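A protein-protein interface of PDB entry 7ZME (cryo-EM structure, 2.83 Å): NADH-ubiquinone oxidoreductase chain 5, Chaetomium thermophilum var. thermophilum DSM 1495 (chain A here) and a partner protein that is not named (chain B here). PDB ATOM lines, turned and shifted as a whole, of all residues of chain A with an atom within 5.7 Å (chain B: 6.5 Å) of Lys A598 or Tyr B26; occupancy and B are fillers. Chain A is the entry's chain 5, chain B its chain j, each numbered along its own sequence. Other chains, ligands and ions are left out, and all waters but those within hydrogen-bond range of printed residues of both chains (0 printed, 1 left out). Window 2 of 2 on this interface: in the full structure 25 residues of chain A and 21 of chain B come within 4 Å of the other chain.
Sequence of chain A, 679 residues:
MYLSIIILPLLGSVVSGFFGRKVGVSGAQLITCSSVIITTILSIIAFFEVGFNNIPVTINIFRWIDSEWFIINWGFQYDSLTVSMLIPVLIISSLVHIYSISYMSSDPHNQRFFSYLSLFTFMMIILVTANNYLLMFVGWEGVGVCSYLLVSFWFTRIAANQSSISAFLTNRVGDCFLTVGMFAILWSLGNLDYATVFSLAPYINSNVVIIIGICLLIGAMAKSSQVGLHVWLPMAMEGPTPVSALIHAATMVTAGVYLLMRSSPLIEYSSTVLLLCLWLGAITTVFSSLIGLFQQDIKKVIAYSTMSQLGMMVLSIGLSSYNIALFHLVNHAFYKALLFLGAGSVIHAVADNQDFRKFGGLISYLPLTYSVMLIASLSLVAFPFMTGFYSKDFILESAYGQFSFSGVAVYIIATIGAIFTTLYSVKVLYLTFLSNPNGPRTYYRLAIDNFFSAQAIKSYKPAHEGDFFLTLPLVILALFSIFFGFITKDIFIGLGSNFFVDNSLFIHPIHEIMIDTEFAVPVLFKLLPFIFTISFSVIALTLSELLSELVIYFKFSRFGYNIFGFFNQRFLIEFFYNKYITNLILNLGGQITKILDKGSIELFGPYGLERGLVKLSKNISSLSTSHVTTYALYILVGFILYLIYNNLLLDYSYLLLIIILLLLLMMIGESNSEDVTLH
The backbone carbonyl oxygen (O) of Glu A602 sits at hydrogen-bond distance from the backbone NH (N) of Tyr A607.
OD1 of Asn B24 is in hydrogen-bond range of NZ of Lys B27 (2.9 Å).
The backbone carbonyl oxygen (O) of Thr A593 sits at hydrogen-bond distance from the backbone NH (N) of Lys A598 (3.0 Å).
The backbone carbonyl oxygen (O) of Ile A595 sits at hydrogen-bond distance from the backbone NH (N) of Ser A600, 2.9 Å away.
Among the printed residues, pairs that only touch across the chains: Tyr A607 with Tyr B26 (3.3 Å), Lys A598 with Tyr B26 (3.5 Å), Gly A599 with Phe B29 (3.5 Å), Ser A600 with Phe B29 (3.5 Å), Lys A594 with Arg B25 (3.6 Å), Lys A598 with Ile B22 (3.7 Å), Ile A595 with Phe B29 (3.7 Å), Tyr A607 with Lys B27 (3.8 Å) and Glu A602 with Tyr B26 (3.9 Å).
Of the printed residues of chain B, Lys A598 touches Ile B22 and Tyr B26.
Of the printed residues of chain A, Tyr B26 touches Lys A598 (3.5 Å), Glu A602 (3.9 Å) and Tyr A607 (3.3 Å).
Printed residues of chain B within 4 Å of Ser A600: Phe B29 (3.5 Å).
Of the printed residues of chain B, Tyr A607 touches Tyr B26 (3.3 Å) and Lys B27 (3.8 Å).
Printed residues of chain B within 4 Å of Ile A595: Phe B29 (3.7 Å).
Of the printed residues of chain B, Lys A594 touches Arg B25.
Printed residues of chain B within 4 Å of Gly A599: Phe B29 (3.5 Å).
Thr A593 touches none of the printed residues of chain B.
The nearest residue of chain B that does not touch Lys A598 is Arg B25 (4.1 Å).
The nearest printed residue of chain A that does not touch Ile B22 is Lys A594 (7.0 Å).
Printed residues of chain A that touch a printed residue of chain B: Lys A594, Ile A595, Lys A598, Gly A599, Ser A600, Glu A602 and Tyr A607.
Hydrophobic or aromatic side chains of chain A that line the printed part of chain B: Tyr A607.
Hydrophobic or aromatic side chains of chain B within 4 Å of the printed part of chain A: Tyr B26 and Phe B29.
Along chain B the printed residues that touch a printed residue of chain A span positions 22 to 29.
Among the printed residues, 9 pairs touch across the chains.
Among the printed residues, no Asp or Glu carboxylate lies within 4 Å of a Lys or Arg side-chain nitrogen of the other chain.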
ATOM      1  N   ILE A 592      21.387 -21.209  19.345  1.00  0.00           N
ATOM      2  CA  ILE A 592      22.427 -22.129  19.796  1.00  0.00           C
ATOM      3  C   ILE A 592      23.607 -21.372  20.392  1.00  0.00           C
ATOM      4  O   ILE A 592      24.133 -21.753  21.443  1.00  0.00           O
ATOM      5  CB  ILE A 592      22.866 -23.049  18.643  1.00  0.00           C
ATOM      6  CG1 ILE A 592      21.651 -23.592  17.898  1.00  0.00           C
ATOM      7  CG2 ILE A 592      23.724 -24.191  19.159  1.00  0.00           C
ATOM      8  CD1 ILE A 592      22.004 -24.348  16.648  1.00  0.00           C
ATOM      9  N   THR A 593      24.051 -20.301  19.730  1.00  0.00           N
ATOM     10  CA  THR A 593      25.203 -19.551  20.229  1.00  0.00           C
ATOM     11  C   THR A 593      24.914 -18.879  21.564  1.00  0.00           C
ATOM     12  O   THR A 593      25.768 -18.876  22.457  1.00  0.00           O
ATOM     13  CB  THR A 593      25.646 -18.504  19.206  1.00  0.00           C
ATOM     14  OG1 THR A 593      24.689 -17.437  19.161  1.00  0.00           O
ATOM     15  CG2 THR A 593      25.821 -19.113  17.835  1.00  0.00           C
ATOM     16  N   LYS A 594      23.725 -18.299  21.721  1.00  0.00           N
ATOM     17  CA  LYS A 594      23.442 -17.472  22.888  1.00  0.00           C
ATOM     18  C   LYS A 594      22.810 -18.261  24.028  1.00  0.00           C
ATOM     19  O   LYS A 594      23.202 -18.100  25.186  1.00  0.00           O
ATOM     20  CB  LYS A 594      22.543 -16.300  22.486  1.00  0.00           C
ATOM     21  CG  LYS A 594      23.170 -15.398  21.443  1.00  0.00           C
ATOM     22  CD  LYS A 594      22.264 -14.237  21.068  1.00  0.00           C
ATOM     23  CE  LYS A 594      21.001 -14.716  20.378  1.00  0.00           C
ATOM     24  NZ  LYS A 594      20.453 -13.696  19.442  1.00  0.00           N
ATOM     25  N   ILE A 595      21.834 -19.113  23.727  1.00  0.00           N
ATOM     26  CA  ILE A 595      21.140 -19.840  24.782  1.00  0.00           C
ATOM     27  C   ILE A 595      21.778 -21.190  25.098  1.00  0.00           C
ATOM     28  O   ILE A 595      21.705 -21.643  26.249  1.00  0.00           O
ATOM     29  CB  ILE A 595      19.656 -20.024  24.417  1.00  0.00           C
ATOM     30  CG1 ILE A 595      19.029 -18.678  24.077  1.00  0.00           C
ATOM     31  CG2 ILE A 595      18.885 -20.674  25.544  1.00  0.00           C
ATOM     32  CD1 ILE A 595      17.725 -18.802  23.352  1.00  0.00           C
ATOM     33  N   LEU A 596      22.413 -21.840  24.125  1.00  0.00           N
ATOM     34  CA  LEU A 596      22.983 -23.167  24.337  1.00  0.00           C
ATOM     35  C   LEU A 596      24.488 -23.104  24.572  1.00  0.00           C
ATOM     36  O   LEU A 596      24.951 -23.465  25.652  1.00  0.00           O
ATOM     37  CB  LEU A 596      22.651 -24.090  23.161  1.00  0.00           C
ATOM     38  CG  LEU A 596      21.315 -24.831  23.220  1.00  0.00           C
ATOM     39  CD1 LEU A 596      21.303 -25.731  24.430  1.00  0.00           C
ATOM     40  CD2 LEU A 596      20.129 -23.890  23.249  1.00  0.00           C
ATOM     41  N   ASP A 597      25.259 -22.681  23.579  1.00  0.00           N
ATOM     42  CA  ASP A 597      26.738 -22.792  23.651  1.00  0.00           C
ATOM     43  C   ASP A 597      27.370 -21.701  24.505  1.00  0.00           C
ATOM     44  O   ASP A 597      28.513 -21.893  24.920  1.00  0.00           O
ATOM     45  CB  ASP A 597      27.314 -22.767  22.235  1.00  0.00           C
ATOM     46  CG  ASP A 597      27.425 -24.122  21.572  1.00  0.00           C
ATOM     47  OD1 ASP A 597      27.230 -25.132  22.274  1.00  0.00           O
ATOM     48  OD2 ASP A 597      27.723 -24.149  20.365  1.00  0.00           O
ATOM     49  N   LYS A 598      26.680 -20.604  24.767  1.00  0.00           N
ATOM     50  CA  LYS A 598      27.189 -19.586  25.717  1.00  0.00           C
ATOM     51  C   LYS A 598      26.103 -19.429  26.773  1.00  0.00           C
ATOM     52  O   LYS A 598      25.910 -18.300  27.247  1.00  0.00           O
ATOM     53  CB  LYS A 598      27.514 -18.284  24.990  1.00  0.00           C
ATOM     54  CG  LYS A 598      28.675 -18.360  24.009  1.00  0.00           C
ATOM     55  CD  LYS A 598      28.924 -17.069  23.266  1.00  0.00           C
ATOM     56  CE  LYS A 598      29.878 -17.231  22.104  1.00  0.00           C
ATOM     57  NZ  LYS A 598      31.140 -17.892  22.515  1.00  0.00           N
ATOM     58  N   GLY A 599      25.379 -20.513  27.069  1.00  0.00           N
ATOM     59  CA  GLY A 599      24.237 -20.441  27.992  1.00  0.00           C
ATOM     60  C   GLY A 599      24.097 -21.654  28.878  1.00  0.00           C
ATOM     61  O   GLY A 599      24.833 -21.734  29.865  1.00  0.00           O
ATOM     62  N   SER A 600      23.152 -22.540  28.573  1.00  0.00           N
ATOM     63  CA  SER A 600      22.896 -23.674  29.452  1.00  0.00           C
ATOM     64  C   SER A 600      24.035 -24.689  29.447  1.00  0.00           C
ATOM     65  O   SER A 600      24.298 -25.326  30.473  1.00  0.00           O
ATOM     66  CB  SER A 600      21.591 -24.341  29.039  1.00  0.00           C
ATOM     67  OG  SER A 600      21.654 -24.785  27.700  1.00  0.00           O
ATOM     68  N   GLU A 602      27.167 -24.068  29.287  1.00  0.00           N
ATOM     69  CA  GLU A 602      28.107 -23.537  30.268  1.00  0.00           C
ATOM     70  C   GLU A 602      27.568 -23.661  31.689  1.00  0.00           C
ATOM     71  O   GLU A 602      28.300 -24.057  32.600  1.00  0.00           O
ATOM     72  CB  GLU A 602      28.432 -22.078  29.945  1.00  0.00           C
ATOM     73  CG  GLU A 602      29.407 -21.865  28.794  1.00  0.00           C
ATOM     74  CD  GLU A 602      30.827 -22.333  29.094  1.00  0.00           C
ATOM     75  OE1 GLU A 602      31.711 -22.117  28.239  1.00  0.00           O
ATOM     76  OE2 GLU A 602      31.081 -22.879  30.184  1.00  0.00           O
ATOM     77  N   TYR A 607      30.963 -23.896  33.873  1.00  0.00           N
ATOM     78  CA  TYR A 607      30.764 -22.676  34.648  1.00  0.00           C
ATOM     79  C   TYR A 607      29.882 -22.918  35.867  1.00  0.00           C
ATOM     80  O   TYR A 607      30.137 -22.362  36.940  1.00  0.00           O
ATOM     81  CB  TYR A 607      30.161 -21.577  33.781  1.00  0.00           C
ATOM     82  CG  TYR A 607      29.977 -20.279  34.534  1.00  0.00           C
ATOM     83  CD1 TYR A 607      31.071 -19.562  34.988  1.00  0.00           C
ATOM     84  CD2 TYR A 607      28.713 -19.779  34.803  1.00  0.00           C
ATOM     85  CE1 TYR A 607      30.917 -18.385  35.675  1.00  0.00           C
ATOM     86  CE2 TYR A 607      28.550 -18.598  35.494  1.00  0.00           C
ATOM     87  CZ  TYR A 607      29.658 -17.906  35.926  1.00  0.00           C
ATOM     88  OH  TYR A 607      29.510 -16.725  36.615  1.00  0.00           O
ATOM     89  N   MET B  21      30.945  -8.169  25.391  1.00  0.00           N
ATOM     90  CA  MET B  21      29.685  -8.719  25.880  1.00  0.00           C
ATOM     91  C   MET B  21      29.476 -10.142  25.386  1.00  0.00           C
ATOM     92  O   MET B  21      29.070 -11.020  26.154  1.00  0.00           O
ATOM     93  CB  MET B  21      28.524  -7.816  25.454  1.00  0.00           C
ATOM     94  CG  MET B  21      27.151  -8.247  25.955  1.00  0.00           C
ATOM     95  SD  MET B  21      26.354  -9.535  24.973  1.00  0.00           S
ATOM     96  CE  MET B  21      25.910  -8.615  23.507  1.00  0.00           C
ATOM     97  N   ILE B  22      29.736 -10.385  24.101  1.00  0.00           N
ATOM     98  CA  ILE B  22      29.581 -11.724  23.545  1.00  0.00           C
ATOM     99  C   ILE B  22      30.559 -12.686  24.205  1.00  0.00           C
ATOM    100  O   ILE B  22      30.223 -13.839  24.495  1.00  0.00           O
ATOM    101  CB  ILE B  22      29.759 -11.680  22.017  1.00  0.00           C
ATOM    102  CG1 ILE B  22      28.573 -10.967  21.369  1.00  0.00           C
ATOM    103  CG2 ILE B  22      29.910 -13.079  21.445  1.00  0.00           C
ATOM    104  CD1 ILE B  22      28.834 -10.522  19.951  1.00  0.00           C
ATOM    105  N   SER B  23      31.783 -12.220  24.464  1.00  0.00           N
ATOM    106  CA  SER B  23      32.779 -13.054  25.126  1.00  0.00           C
ATOM    107  C   SER B  23      32.369 -13.394  26.551  1.00  0.00           C
ATOM    108  O   SER B  23      32.621 -14.505  27.029  1.00  0.00           O
ATOM    109  CB  SER B  23      34.134 -12.353  25.121  1.00  0.00           C
ATOM    110  OG  SER B  23      35.108 -13.134  25.788  1.00  0.00           O
ATOM    111  N   ASN B  24      31.751 -12.446  27.252  1.00  0.00           N
ATOM    112  CA  ASN B  24      31.427 -12.590  28.662  1.00  0.00           C
ATOM    113  C   ASN B  24      29.998 -13.056  28.895  1.00  0.00           C
ATOM    114  O   ASN B  24      29.558 -13.117  30.046  1.00  0.00           O
ATOM    115  CB  ASN B  24      31.657 -11.264  29.386  1.00  0.00           C
ATOM    116  CG  ASN B  24      33.119 -10.923  29.521  1.00  0.00           C
ATOM    117  OD1 ASN B  24      33.903 -11.706  30.047  1.00  0.00           O
ATOM    118  ND2 ASN B  24      33.491  -9.739  29.065  1.00  0.00           N
ATOM    119  N   ARG B  25      29.271 -13.398  27.831  1.00  0.00           N
ATOM    120  CA  ARG B  25      27.833 -13.629  27.933  1.00  0.00           C
ATOM    121  C   ARG B  25      27.495 -14.818  28.827  1.00  0.00           C
ATOM    122  O   ARG B  25      26.409 -14.858  29.415  1.00  0.00           O
ATOM    123  CB  ARG B  25      27.248 -13.839  26.538  1.00  0.00           C
ATOM    124  CG  ARG B  25      25.743 -13.851  26.507  1.00  0.00           C
ATOM    125  CD  ARG B  25      25.197 -14.100  25.119  1.00  0.00           C
ATOM    126  NE  ARG B  25      23.746 -14.231  25.163  1.00  0.00           N
ATOM    127  CZ  ARG B  25      22.901 -13.221  25.003  1.00  0.00           C
ATOM    128  NH1 ARG B  25      23.363 -12.004  24.763  1.00  0.00           N
ATOM    129  NH2 ARG B  25      21.595 -13.427  25.071  1.00  0.00           N
ATOM    130  N   TYR B  26      28.405 -15.786  28.947  1.00  0.00           N
ATOM    131  CA  TYR B  26      28.082 -17.033  29.631  1.00  0.00           C
ATOM    132  C   TYR B  26      27.799 -16.827  31.116  1.00  0.00           C
ATOM    133  O   TYR B  26      27.091 -17.633  31.726  1.00  0.00           O
ATOM    134  CB  TYR B  26      29.221 -18.036  29.436  1.00  0.00           C
ATOM    135  CG  TYR B  26      30.475 -17.713  30.220  1.00  0.00           C
ATOM    136  CD1 TYR B  26      31.387 -16.778  29.756  1.00  0.00           C
ATOM    137  CD2 TYR B  26      30.745 -18.348  31.418  1.00  0.00           C
ATOM    138  CE1 TYR B  26      32.526 -16.484  30.466  1.00  0.00           C
ATOM    139  CE2 TYR B  26      31.882 -18.058  32.132  1.00  0.00           C
ATOM    140  CZ  TYR B  26      32.769 -17.130  31.655  1.00  0.00           C
ATOM    141  OH  TYR B  26      33.907 -16.849  32.374  1.00  0.00           O
ATOM    142  N   LYS B  27      28.339 -15.761  31.713  1.00  0.00           N
ATOM    143  CA  LYS B  27      28.184 -15.529  33.145  1.00  0.00           C
ATOM    144  C   LYS B  27      26.781 -15.107  33.547  1.00  0.00           C
ATOM    145  O   LYS B  27      26.455 -15.179  34.736  1.00  0.00           O
ATOM    146  CB  LYS B  27      29.156 -14.455  33.628  1.00  0.00           C
ATOM    147  CG  LYS B  27      30.521 -14.461  32.993  1.00  0.00           C
ATOM    148  CD  LYS B  27      31.514 -13.824  33.944  1.00  0.00           C
ATOM    149  CE  LYS B  27      32.945 -14.146  33.575  1.00  0.00           C
ATOM    150  NZ  LYS B  27      33.463 -13.249  32.515  1.00  0.00           N
ATOM    151  N   TYR B  28      25.952 -14.659  32.610  1.00  0.00           N
ATOM    152  CA  TYR B  28      24.681 -14.026  32.934  1.00  0.00           C
ATOM    153  C   TYR B  28      23.488 -14.889  32.568  1.00  0.00           C
ATOM    154  O   TYR B  28      22.344 -14.457  32.735  1.00  0.00           O
ATOM    155  CB  TYR B  28      24.592 -12.669  32.239  1.00  0.00           C
ATOM    156  CG  TYR B  28      25.733 -11.756  32.600  1.00  0.00           C
ATOM    157  CD1 TYR B  28      25.716 -11.030  33.775  1.00  0.00           C
ATOM    158  CD2 TYR B  28      26.839 -11.638  31.777  1.00  0.00           C
ATOM    159  CE1 TYR B  28      26.756 -10.198  34.110  1.00  0.00           C
ATOM    160  CE2 TYR B  28      27.886 -10.814  32.109  1.00  0.00           C
ATOM    161  CZ  TYR B  28      27.839 -10.095  33.277  1.00  0.00           C
ATOM    162  OH  TYR B  28      28.880  -9.266  33.613  1.00  0.00           O
ATOM    163  N   PHE B  29      23.729 -16.096  32.080  1.00  0.00           N
ATOM    164  CA  PHE B  29      22.651 -17.005  31.734  1.00  0.00           C
ATOM    165  C   PHE B  29      21.899 -17.450  32.984  1.00  0.00           C
ATOM    166  O   PHE B  29      22.500 -17.696  34.032  1.00  0.00           O
ATOM    167  CB  PHE B  29      23.225 -18.212  31.004  1.00  0.00           C
ATOM    168  CG  PHE B  29      22.252 -19.317  30.817  1.00  0.00           C
ATOM    169  CD1 PHE B  29      21.422 -19.326  29.720  1.00  0.00           C
ATOM    170  CD2 PHE B  29      22.153 -20.340  31.739  1.00  0.00           C
ATOM    171  CE1 PHE B  29      20.539 -20.329  29.541  1.00  0.00           C
ATOM    172  CE2 PHE B  29      21.247 -21.345  31.565  1.00  0.00           C
ATOM    173  CZ  PHE B  29      20.439 -21.342  30.464  1.00  0.00           C
